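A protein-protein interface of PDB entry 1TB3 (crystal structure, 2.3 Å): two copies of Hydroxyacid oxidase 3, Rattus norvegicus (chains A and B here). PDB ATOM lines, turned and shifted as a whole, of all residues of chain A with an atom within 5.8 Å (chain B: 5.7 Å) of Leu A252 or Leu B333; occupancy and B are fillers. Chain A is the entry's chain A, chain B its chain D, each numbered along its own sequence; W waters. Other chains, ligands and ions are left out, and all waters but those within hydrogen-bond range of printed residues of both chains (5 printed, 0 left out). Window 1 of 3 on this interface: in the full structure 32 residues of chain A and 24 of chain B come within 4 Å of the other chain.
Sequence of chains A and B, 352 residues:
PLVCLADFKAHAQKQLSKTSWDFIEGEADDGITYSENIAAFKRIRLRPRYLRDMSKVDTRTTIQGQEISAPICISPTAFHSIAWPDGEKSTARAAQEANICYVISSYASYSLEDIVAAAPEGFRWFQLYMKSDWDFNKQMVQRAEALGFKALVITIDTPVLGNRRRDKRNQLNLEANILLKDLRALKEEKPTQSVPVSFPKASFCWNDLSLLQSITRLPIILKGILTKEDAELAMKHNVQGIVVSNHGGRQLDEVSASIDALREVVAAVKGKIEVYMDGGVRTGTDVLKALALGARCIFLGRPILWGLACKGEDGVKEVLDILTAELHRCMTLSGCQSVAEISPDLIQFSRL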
ATOM      1  N   ALA A  28       9.540  -2.996   3.793  1.00  0.00           N
ATOM      2  CA  ALA A  28       9.676  -1.833   4.671  1.00  0.00           C
ATOM      3  C   ALA A  28      10.363  -0.683   3.970  1.00  0.00           C
ATOM      4  O   ALA A  28      11.280  -0.883   3.176  1.00  0.00           O
ATOM      5  CB  ALA A  28      10.448  -2.202   5.932  1.00  0.00           C
ATOM      6  N   ASP A  29       9.884   0.523   4.254  1.00  0.00           N
ATOM      7  CA  ASP A  29      10.439   1.744   3.690  1.00  0.00           C
ATOM      8  C   ASP A  29      10.665   1.726   2.167  1.00  0.00           C
ATOM      9  O   ASP A  29       9.722   1.522   1.406  1.00  0.00           O
ATOM     10  CB  ASP A  29      11.720   2.070   4.471  1.00  0.00           C
ATOM     11  CG  ASP A  29      11.456   2.188   5.978  1.00  0.00           C
ATOM     12  OD1 ASP A  29      10.818   3.184   6.384  1.00  0.00           O
ATOM     13  OD2 ASP A  29      11.848   1.274   6.752  1.00  0.00           O
ATOM     14  N   THR A  33      15.853  -4.292   0.672  1.00  0.00           N
ATOM     15  CA  THR A  33      16.178  -5.658   1.055  1.00  0.00           C
ATOM     16  C   THR A  33      15.236  -6.729   0.506  1.00  0.00           C
ATOM     17  O   THR A  33      15.658  -7.854   0.257  1.00  0.00           O
ATOM     18  CB  THR A  33      16.255  -5.766   2.576  1.00  0.00           C
ATOM     19  OG1 THR A  33      17.157  -4.765   3.059  1.00  0.00           O
ATOM     20  CG2 THR A  33      16.748  -7.161   3.004  1.00  0.00           C
ATOM     21  N   ASP A 157      14.537  -9.708  15.590  1.00  0.00           N
ATOM     22  CA  ASP A 157      14.604  -8.495  14.769  1.00  0.00           C
ATOM     23  C   ASP A 157      13.317  -7.685  14.742  1.00  0.00           C
ATOM     24  O   ASP A 157      13.107  -6.864  13.850  1.00  0.00           O
ATOM     25  CB  ASP A 157      15.018  -8.855  13.335  1.00  0.00           C
ATOM     26  CG  ASP A 157      14.047  -9.825  12.657  1.00  0.00           C
ATOM     27  OD1 ASP A 157      14.439 -10.407  11.625  1.00  0.00           O
ATOM     28  OD2 ASP A 157      12.902 -10.000  13.135  1.00  0.00           O
ATOM     29  N   THR A 158      12.460  -7.892  15.731  1.00  0.00           N
ATOM     30  CA  THR A 158      11.192  -7.183  15.752  1.00  0.00           C
ATOM     31  C   THR A 158      10.842  -6.560  17.107  1.00  0.00           C
ATOM     32  O   THR A 158       9.769  -6.800  17.656  1.00  0.00           O
ATOM     33  CB  THR A 158      10.055  -8.132  15.297  1.00  0.00           C
ATOM     34  OG1 THR A 158      10.448  -8.786  14.083  1.00  0.00           O
ATOM     35  CG2 THR A 158       8.781  -7.355  15.025  1.00  0.00           C
ATOM     36  N   PRO A 159      11.759  -5.764  17.671  1.00  0.00           N
ATOM     37  CA  PRO A 159      11.464  -5.138  18.961  1.00  0.00           C
ATOM     38  C   PRO A 159      10.308  -4.156  18.756  1.00  0.00           C
ATOM     39  O   PRO A 159       9.584  -3.817  19.685  1.00  0.00           O
ATOM     40  CB  PRO A 159      12.783  -4.451  19.318  1.00  0.00           C
ATOM     41  CG  PRO A 159      13.361  -4.115  17.975  1.00  0.00           C
ATOM     42  CD  PRO A 159      13.103  -5.386  17.199  1.00  0.00           C
ATOM     43  N   VAL A 160      10.156  -3.702  17.517  1.00  0.00           N
ATOM     44  CA  VAL A 160       9.080  -2.802  17.137  1.00  0.00           C
ATOM     45  C   VAL A 160       8.780  -3.209  15.693  1.00  0.00           C
ATOM     46  O   VAL A 160       9.642  -3.785  15.032  1.00  0.00           O
ATOM     47  CB  VAL A 160       9.524  -1.322  17.212  1.00  0.00           C
ATOM     48  CG1 VAL A 160      10.542  -1.005  16.124  1.00  0.00           C
ATOM     49  CG2 VAL A 160       8.332  -0.430  17.084  1.00  0.00           C
ATOM     50  N   LEU A 161       7.571  -2.942  15.207  1.00  0.00           N
ATOM     51  CA  LEU A 161       7.221  -3.320  13.839  1.00  0.00           C
ATOM     52  C   LEU A 161       7.859  -2.452  12.766  1.00  0.00           C
ATOM     53  O   LEU A 161       8.031  -1.246  12.952  1.00  0.00           O
ATOM     54  CB  LEU A 161       5.704  -3.298  13.638  1.00  0.00           C
ATOM     55  CG  LEU A 161       4.892  -4.456  14.223  1.00  0.00           C
ATOM     56  CD1 LEU A 161       3.423  -4.271  13.869  1.00  0.00           C
ATOM     57  CD2 LEU A 161       5.401  -5.786  13.678  1.00  0.00           C
ATOM     58  N   GLY A 162       8.180  -3.084  11.638  1.00  0.00           N
ATOM     59  CA  GLY A 162       8.776  -2.386  10.513  1.00  0.00           C
ATOM     60  C   GLY A 162       7.791  -1.409   9.895  1.00  0.00           C
ATOM     61  O   GLY A 162       6.579  -1.546  10.063  1.00  0.00           O
ATOM     62  N   ASN A 246      16.402 -11.616   7.615  1.00  0.00           N
ATOM     63  CA  ASN A 246      16.190 -10.179   7.731  1.00  0.00           C
ATOM     64  C   ASN A 246      14.676  -9.942   7.711  1.00  0.00           C
ATOM     65  O   ASN A 246      14.202  -8.875   7.299  1.00  0.00           O
ATOM     66  CB  ASN A 246      16.863  -9.397   6.598  1.00  0.00           C
ATOM     67  CG  ASN A 246      16.578  -9.977   5.221  1.00  0.00           C
ATOM     68  OD1 ASN A 246      15.458 -10.387   4.918  1.00  0.00           O
ATOM     69  ND2 ASN A 246      17.601  -9.994   4.369  1.00  0.00           N
ATOM     70  N   GLY A 249      12.808  -8.496   4.625  1.00  0.00           N
ATOM     71  CA  GLY A 249      12.843  -7.084   4.298  1.00  0.00           C
ATOM     72  C   GLY A 249      11.625  -6.325   4.800  1.00  0.00           C
ATOM     73  O   GLY A 249      11.321  -5.235   4.304  1.00  0.00           O
ATOM     74  N   ARG A 250      10.924  -6.896   5.780  1.00  0.00           N
ATOM     75  CA  ARG A 250       9.737  -6.266   6.357  1.00  0.00           C
ATOM     76  C   ARG A 250      10.058  -5.484   7.635  1.00  0.00           C
ATOM     77  O   ARG A 250       9.181  -4.835   8.202  1.00  0.00           O
ATOM     78  CB  ARG A 250       8.688  -7.330   6.677  1.00  0.00           C
ATOM     79  CG  ARG A 250       8.249  -8.163   5.465  1.00  0.00           C
ATOM     80  CD  ARG A 250       7.615  -9.473   5.896  1.00  0.00           C
ATOM     81  NE  ARG A 250       6.385  -9.287   6.664  1.00  0.00           N
ATOM     82  CZ  ARG A 250       5.194  -9.042   6.119  1.00  0.00           C
ATOM     83  NH1 ARG A 250       5.066  -8.952   4.796  1.00  0.00           N
ATOM     84  NH2 ARG A 250       4.129  -8.900   6.894  1.00  0.00           N
ATOM     85  N   GLN A 251      11.310  -5.545   8.086  1.00  0.00           N
ATOM     86  CA  GLN A 251      11.713  -4.857   9.306  1.00  0.00           C
ATOM     87  C   GLN A 251      12.728  -3.746   9.066  1.00  0.00           C
ATOM     88  O   GLN A 251      12.365  -2.692   8.550  1.00  0.00           O
ATOM     89  CB  GLN A 251      12.246  -5.874  10.314  1.00  0.00           C
ATOM     90  CG  GLN A 251      11.141  -6.720  10.936  1.00  0.00           C
ATOM     91  CD  GLN A 251      10.202  -5.896  11.812  1.00  0.00           C
ATOM     92  OE1 GLN A 251      10.624  -5.320  12.814  1.00  0.00           O
ATOM     93  NE2 GLN A 251       8.928  -5.838  11.438  1.00  0.00           N
ATOM     94  N   LEU A 252      13.982  -3.944   9.465  1.00  0.00           N
ATOM     95  CA  LEU A 252      14.992  -2.912   9.227  1.00  0.00           C
ATOM     96  C   LEU A 252      15.391  -3.086   7.764  1.00  0.00           C
ATOM     97  O   LEU A 252      15.935  -4.116   7.392  1.00  0.00           O
ATOM     98  CB  LEU A 252      16.224  -3.125  10.112  1.00  0.00           C
ATOM     99  CG  LEU A 252      17.067  -1.903  10.508  1.00  0.00           C
ATOM    100  CD1 LEU A 252      18.516  -2.310  10.606  1.00  0.00           C
ATOM    101  CD2 LEU A 252      16.918  -0.780   9.510  1.00  0.00           C
ATOM    102  N   ASP A 253      15.120  -2.098   6.925  1.00  0.00           N
ATOM    103  CA  ASP A 253      15.465  -2.231   5.513  1.00  0.00           C
ATOM    104  C   ASP A 253      16.904  -1.810   5.235  1.00  0.00           C
ATOM    105  O   ASP A 253      17.540  -1.147   6.049  1.00  0.00           O
ATOM    106  CB  ASP A 253      14.497  -1.406   4.653  1.00  0.00           C
ATOM    107  CG  ASP A 253      14.624  -1.710   3.164  1.00  0.00           C
ATOM    108  OD1 ASP A 253      14.810  -2.897   2.805  1.00  0.00           O
ATOM    109  OD2 ASP A 253      14.524  -0.765   2.352  1.00  0.00           O
ATOM    110  N   GLU A 254      17.402  -2.211   4.074  1.00  0.00           N
ATOM    111  CA  GLU A 254      18.745  -1.887   3.635  1.00  0.00           C
ATOM    112  C   GLU A 254      19.845  -2.581   4.433  1.00  0.00           C
ATOM    113  O   GLU A 254      20.943  -2.055   4.603  1.00  0.00           O
ATOM    114  CB  GLU A 254      18.931  -0.359   3.599  1.00  0.00           C
ATOM    115  CG  GLU A 254      17.775   0.326   2.868  1.00  0.00           C
ATOM    116  CD  GLU A 254      18.050   1.762   2.471  1.00  0.00           C
ATOM    117  OE1 GLU A 254      17.070   2.488   2.184  1.00  0.00           O
ATOM    118  OE2 GLU A 254      19.230   2.169   2.427  1.00  0.00           O
ATOM    119  N   VAL A 255      19.533  -3.772   4.933  1.00  0.00           N
ATOM    120  CA  VAL A 255      20.515  -4.585   5.638  1.00  0.00           C
ATOM    121  C   VAL A 255      20.947  -5.595   4.564  1.00  0.00           C
ATOM    122  O   VAL A 255      20.410  -5.578   3.451  1.00  0.00           O
ATOM    123  CB  VAL A 255      19.904  -5.347   6.838  1.00  0.00           C
ATOM    124  CG1 VAL A 255      19.361  -4.348   7.861  1.00  0.00           C
ATOM    125  CG2 VAL A 255      18.806  -6.305   6.359  1.00  0.00           C
ATOM    126  N   LEU B  46      23.429  -1.987   6.230  1.00  0.00           N
ATOM    127  CA  LEU B  46      23.428  -1.818   7.671  1.00  0.00           C
ATOM    128  C   LEU B  46      23.700  -3.127   8.405  1.00  0.00           C
ATOM    129  O   LEU B  46      23.334  -4.199   7.928  1.00  0.00           O
ATOM    130  CB  LEU B  46      22.075  -1.259   8.120  1.00  0.00           C
ATOM    131  CG  LEU B  46      21.744   0.163   7.657  1.00  0.00           C
ATOM    132  CD1 LEU B  46      20.293   0.497   7.994  1.00  0.00           C
ATOM    133  CD2 LEU B  46      22.701   1.154   8.315  1.00  0.00           C
ATOM    134  N   PRO B  48      22.739  -4.526  11.889  1.00  0.00           N
ATOM    135  CA  PRO B  48      22.018  -4.385  13.154  1.00  0.00           C
ATOM    136  C   PRO B  48      22.504  -5.283  14.286  1.00  0.00           C
ATOM    137  O   PRO B  48      23.023  -6.370  14.058  1.00  0.00           O
ATOM    138  CB  PRO B  48      20.580  -4.696  12.757  1.00  0.00           C
ATOM    139  CG  PRO B  48      20.766  -5.797  11.770  1.00  0.00           C
ATOM    140  CD  PRO B  48      21.947  -5.304  10.917  1.00  0.00           C
ATOM    141  N   ARG B  49      22.323  -4.807  15.512  1.00  0.00           N
ATOM    142  CA  ARG B  49      22.687  -5.556  16.704  1.00  0.00           C
ATOM    143  C   ARG B  49      21.393  -5.700  17.494  1.00  0.00           C
ATOM    144  O   ARG B  49      20.835  -4.718  17.986  1.00  0.00           O
ATOM    145  CB  ARG B  49      23.744  -4.796  17.506  1.00  0.00           C
ATOM    146  CG  ARG B  49      25.056  -4.572  16.738  1.00  0.00           C
ATOM    147  CD  ARG B  49      25.576  -5.897  16.153  1.00  0.00           C
ATOM    148  NE  ARG B  49      25.714  -6.921  17.187  1.00  0.00           N
ATOM    149  CZ  ARG B  49      26.664  -6.922  18.121  1.00  0.00           C
ATOM    150  NH1 ARG B  49      27.572  -5.954  18.156  1.00  0.00           N
ATOM    151  NH2 ARG B  49      26.700  -7.888  19.026  1.00  0.00           N
ATOM    152  N   TYR B  50      20.915  -6.929  17.612  1.00  0.00           N
ATOM    153  CA  TYR B  50      19.652  -7.182  18.287  1.00  0.00           C
ATOM    154  C   TYR B  50      19.742  -7.588  19.754  1.00  0.00           C
ATOM    155  O   TYR B  50      20.823  -7.731  20.314  1.00  0.00           O
ATOM    156  CB  TYR B  50      18.885  -8.248  17.504  1.00  0.00           C
ATOM    157  CG  TYR B  50      18.571  -7.858  16.069  1.00  0.00           C
ATOM    158  CD1 TYR B  50      19.010  -8.644  15.000  1.00  0.00           C
ATOM    159  CD2 TYR B  50      17.792  -6.739  15.781  1.00  0.00           C
ATOM    160  CE1 TYR B  50      18.678  -8.330  13.684  1.00  0.00           C
ATOM    161  CE2 TYR B  50      17.450  -6.416  14.464  1.00  0.00           C
ATOM    162  CZ  TYR B  50      17.896  -7.218  13.425  1.00  0.00           C
ATOM    163  OH  TYR B  50      17.539  -6.921  12.133  1.00  0.00           O
ATOM    164  N   MET B  54      16.031  -1.662  24.127  1.00  0.00           N
ATOM    165  CA  MET B  54      15.683  -0.469  23.367  1.00  0.00           C
ATOM    166  C   MET B  54      14.385   0.160  23.846  1.00  0.00           C
ATOM    167  O   MET B  54      13.673   0.783  23.065  1.00  0.00           O
ATOM    168  CB  MET B  54      15.551  -0.819  21.882  1.00  0.00           C
ATOM    169  CG  MET B  54      16.837  -1.291  21.231  1.00  0.00           C
ATOM    170  SD  MET B  54      18.125  -0.026  21.253  1.00  0.00           S
ATOM    171  CE  MET B  54      19.254  -0.713  22.444  1.00  0.00           C
ATOM    172  N   THR B 285      16.707   5.517   7.680  1.00  0.00           N
ATOM    173  CA  THR B 285      18.050   4.961   7.605  1.00  0.00           C
ATOM    174  C   THR B 285      19.069   5.877   6.919  1.00  0.00           C
ATOM    175  O   THR B 285      20.272   5.712   7.132  1.00  0.00           O
ATOM    176  CB  THR B 285      18.056   3.572   6.912  1.00  0.00           C
ATOM    177  OG1 THR B 285      17.463   3.676   5.613  1.00  0.00           O
ATOM    178  CG2 THR B 285      17.292   2.558   7.757  1.00  0.00           C
ATOM    179  N   LEU B 288      20.301   7.759   9.721  1.00  0.00           N
ATOM    180  CA  LEU B 288      21.087   6.820  10.525  1.00  0.00           C
ATOM    181  C   LEU B 288      22.488   6.663   9.955  1.00  0.00           C
ATOM    182  O   LEU B 288      23.473   6.716  10.690  1.00  0.00           O
ATOM    183  CB  LEU B 288      20.424   5.438  10.542  1.00  0.00           C
ATOM    184  CG  LEU B 288      20.443   4.541  11.791  1.00  0.00           C
ATOM    185  CD1 LEU B 288      20.493   3.098  11.347  1.00  0.00           C
ATOM    186  CD2 LEU B 288      21.619   4.842  12.670  1.00  0.00           C
ATOM    187  N   HIS B 328      13.818   7.196  14.704  1.00  0.00           N
ATOM    188  CA  HIS B 328      13.553   6.580  15.987  1.00  0.00           C
ATOM    189  C   HIS B 328      13.332   5.086  15.787  1.00  0.00           C
ATOM    190  O   HIS B 328      13.783   4.265  16.594  1.00  0.00           O
ATOM    191  CB  HIS B 328      12.321   7.229  16.631  1.00  0.00           C
ATOM    192  CG  HIS B 328      11.977   6.672  17.975  1.00  0.00           C
ATOM    193  ND1 HIS B 328      11.425   5.420  18.143  1.00  0.00           N
ATOM    194  CD2 HIS B 328      12.122   7.189  19.217  1.00  0.00           C
ATOM    195  CE1 HIS B 328      11.243   5.191  19.432  1.00  0.00           C
ATOM    196  NE2 HIS B 328      11.657   6.250  20.105  1.00  0.00           N
ATOM    197  N   ARG B 329      12.649   4.738  14.697  1.00  0.00           N
ATOM    198  CA  ARG B 329      12.364   3.341  14.407  1.00  0.00           C
ATOM    199  C   ARG B 329      13.611   2.557  13.999  1.00  0.00           C
ATOM    200  O   ARG B 329      13.863   1.476  14.539  1.00  0.00           O
ATOM    201  CB  ARG B 329      11.269   3.228  13.331  1.00  0.00           C
ATOM    202  CG  ARG B 329      10.906   1.779  12.922  1.00  0.00           C
ATOM    203  CD  ARG B 329       9.496   1.709  12.324  1.00  0.00           C
ATOM    204  NE  ARG B 329       9.287   2.841  11.438  1.00  0.00           N
ATOM    205  CZ  ARG B 329       8.302   3.723  11.559  1.00  0.00           C
ATOM    206  NH1 ARG B 329       7.405   3.609  12.526  1.00  0.00           N
ATOM    207  NH2 ARG B 329       8.241   4.746  10.727  1.00  0.00           N
ATOM    208  N   CYS B 330      14.405   3.074  13.062  1.00  0.00           N
ATOM    209  CA  CYS B 330      15.591   2.315  12.661  1.00  0.00           C
ATOM    210  C   CYS B 330      16.658   2.261  13.759  1.00  0.00           C
ATOM    211  O   CYS B 330      17.467   1.317  13.799  1.00  0.00           O
ATOM    212  CB  CYS B 330      16.183   2.838  11.349  1.00  0.00           C
ATOM    213  SG  CYS B 330      16.776   4.513  11.325  1.00  0.00           S
ATOM    214  N   MET B 331      16.667   3.262  14.645  1.00  0.00           N
ATOM    215  CA  MET B 331      17.610   3.255  15.765  1.00  0.00           C
ATOM    216  C   MET B 331      17.193   2.103  16.688  1.00  0.00           C
ATOM    217  O   MET B 331      18.033   1.337  17.159  1.00  0.00           O
ATOM    218  CB  MET B 331      17.562   4.580  16.536  1.00  0.00           C
ATOM    219  CG  MET B 331      18.304   5.723  15.860  1.00  0.00           C
ATOM    220  SD  MET B 331      18.134   7.296  16.738  1.00  0.00           S
ATOM    221  CE  MET B 331      19.070   6.860  18.240  1.00  0.00           C
ATOM    222  N   THR B 332      15.886   1.979  16.919  1.00  0.00           N
ATOM    223  CA  THR B 332      15.347   0.925  17.770  1.00  0.00           C
ATOM    224  C   THR B 332      15.715  -0.433  17.196  1.00  0.00           C
ATOM    225  O   THR B 332      16.263  -1.281  17.896  1.00  0.00           O
ATOM    226  CB  THR B 332      13.804   1.007  17.869  1.00  0.00           C
ATOM    227  OG1 THR B 332      13.417   2.286  18.391  1.00  0.00           O
ATOM    228  CG2 THR B 332      13.268  -0.093  18.784  1.00  0.00           C
ATOM    229  N   LEU B 333      15.407  -0.621  15.915  1.00  0.00           N
ATOM    230  CA  LEU B 333      15.684  -1.865  15.207  1.00  0.00           C
ATOM    231  C   LEU B 333      17.174  -2.214  15.118  1.00  0.00           C
ATOM    232  O   LEU B 333      17.554  -3.369  15.301  1.00  0.00           O
ATOM    233  CB  LEU B 333      15.097  -1.795  13.790  1.00  0.00           C
ATOM    234  CG  LEU B 333      13.729  -2.409  13.450  1.00  0.00           C
ATOM    235  CD1 LEU B 333      12.957  -2.819  14.687  1.00  0.00           C
ATOM    236  CD2 LEU B 333      12.949  -1.413  12.633  1.00  0.00           C
ATOM    237  N   SER B 334      18.017  -1.222  14.839  1.00  0.00           N
ATOM    238  CA  SER B 334      19.450  -1.476  14.697  1.00  0.00           C
ATOM    239  C   SER B 334      20.205  -1.612  16.018  1.00  0.00           C
ATOM    240  O   SER B 334      21.341  -2.082  16.031  1.00  0.00           O
ATOM    241  CB  SER B 334      20.103  -0.383  13.844  1.00  0.00           C
ATOM    242  OG  SER B 334      20.047   0.868  14.504  1.00  0.00           O
ATOM    243  N   GLY B 335      19.581  -1.198  17.118  1.00  0.00           N
ATOM    244  CA  GLY B 335      20.222  -1.318  18.420  1.00  0.00           C
ATOM    245  C   GLY B 335      20.963  -0.092  18.919  1.00  0.00           C
ATOM    246  O   GLY B 335      21.952  -0.216  19.637  1.00  0.00           O
HETATM  247  O   HOH W   1      14.933  -5.380  12.058  1.00  0.00           O
HETATM  248  O   HOH W   2      11.128   3.642   9.250  1.00  0.00           O
HETATM  249  O   HOH W   3       7.319   1.029  14.353  1.00  0.00           O
HETATM  250  O   HOH W   4      19.261   4.518   3.989  1.00  0.00           O
HETATM  251  O   HOH W   5      16.854  -9.110  10.724  1.00  0.00           O
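Of the 17 printed residues of chain A, 9 touch a printed residue of chain B. Printed residues of chain A that touch a printed residue of chain B: Asp A157, Pro A159, Val A160, Leu A161, Gln A251, Leu A252, Asp A253, Glu A254 and Val A255. Along chain A the printed residues that touch a printed residue of chain B span positions 157 to 255. Of the 15 printed residues of chain B, 7 touch a printed residue of chain A. Printed residues of chain B that touch a printed residue of chain A: Leu B46, Pro B48, Tyr B50, Thr B285, Arg B329, Thr B332 and Leu B333. Along chain B the printed residues that touch a printed residue of chain A span positions 46 to 333. Among the printed residues, 14 pairs touch across the chains. Among the printed residues, no Asp or Glu carboxylate lies within 4 Å of a Lys or Arg side-chain nitrogen of the other chain.
The backbone carbonyl oxygen (O) of Glu A254 lies within hydrogen-bond range of the backbone NH (N) of Leu B46, at 3.0 Å.
Asp A29 touches none of the printed residues of chain B. Leu A252 touches just these residues of chain B: Leu B46 (3.9 Å), Pro B48 (3.8 Å), Thr B285 (3.8 Å) and Leu B333 (3.8 Å). Printed residues of chain A within 4 Å of Pro B48: Leu A252 (3.8 Å). Of the printed residues of chain A, Tyr B50 touches Asp A157 (3.3 Å). Printed residues of chain A within 4 Å of Thr B285: Leu A252 and Glu A254. Leu B333 touches just these residues of chain A: Pro A159, Val A160, Gln A251 and Leu A252. The nearest residue of chain A that does not touch Leu B333 is Asp A157 (4.1 Å). The nearest printed residue of chain A that does not touch Arg B329 is Val A160 (4.3 Å).
Water W4 bridges OG1 of Thr B285 (2.6 Å) and OE2 of Glu A254 (2.8 Å). Water W5 bridges the side-chain hydroxyl of Tyr B50 (2.7 Å) and the side-chain carboxylate of Asp A157 (2.9 Å). Water W3 bridges O of Leu A161 and NH1 of Arg B329. Water W2 bridges the side-chain carboxylate of Asp A29 (2.9 Å) and the guanidinium group of Arg B329 (3.0 Å). Water W1 lies within hydrogen-bond range of O of Asp A157 (3.0 Å), OH of Tyr B50 (3.0 Å) and N of Leu A252 (3.1 Å).
No position is printed for both chains.
Tyr B50 touches Asp A157 (CZ to CB, 3.3 Å). Pro A159 touches Leu B333 (CG to CD1, 3.6 Å). Val A160 touches Thr B332 (CG1 to CG2, 3.9 Å). Leu A161 touches Arg B329. Leu B333 touches Gln A251. Pro B48 touches Leu A252 (CB to CD1, 3.8 Å). CG2 of Thr B285 touches CD2 of Leu A252, 3.8 Å away. Leu A252 touches Leu B333 (CG to CB, 3.8 Å). Asp A253 touches Leu B46. Thr B285 touches Glu A254 (OG1 to OE1, 3.7 Å).
The side-chain carboxylate of Asp A253 is in hydrogen-bond range of the backbone NH of Thr A33. N of Val A255 sits at hydrogen-bond distance from OG1 of Thr A33 (3.2 Å). The backbone NH of Thr B285 is in hydrogen-bond range of the side-chain sulfur of Cys B330 (3.8 Å). O of Asp A157 lies close to OE1 of Gln A251 (3.1 Å). The side-chain hydroxyl (OG1) of Thr A158 lies within hydrogen-bond range of the side-chain carboxylate (OD2) of Asp A157, 2.9 Å away. OG1 of Thr A33 is in hydrogen-bond range of N of Glu A254, 2.8 Å away.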
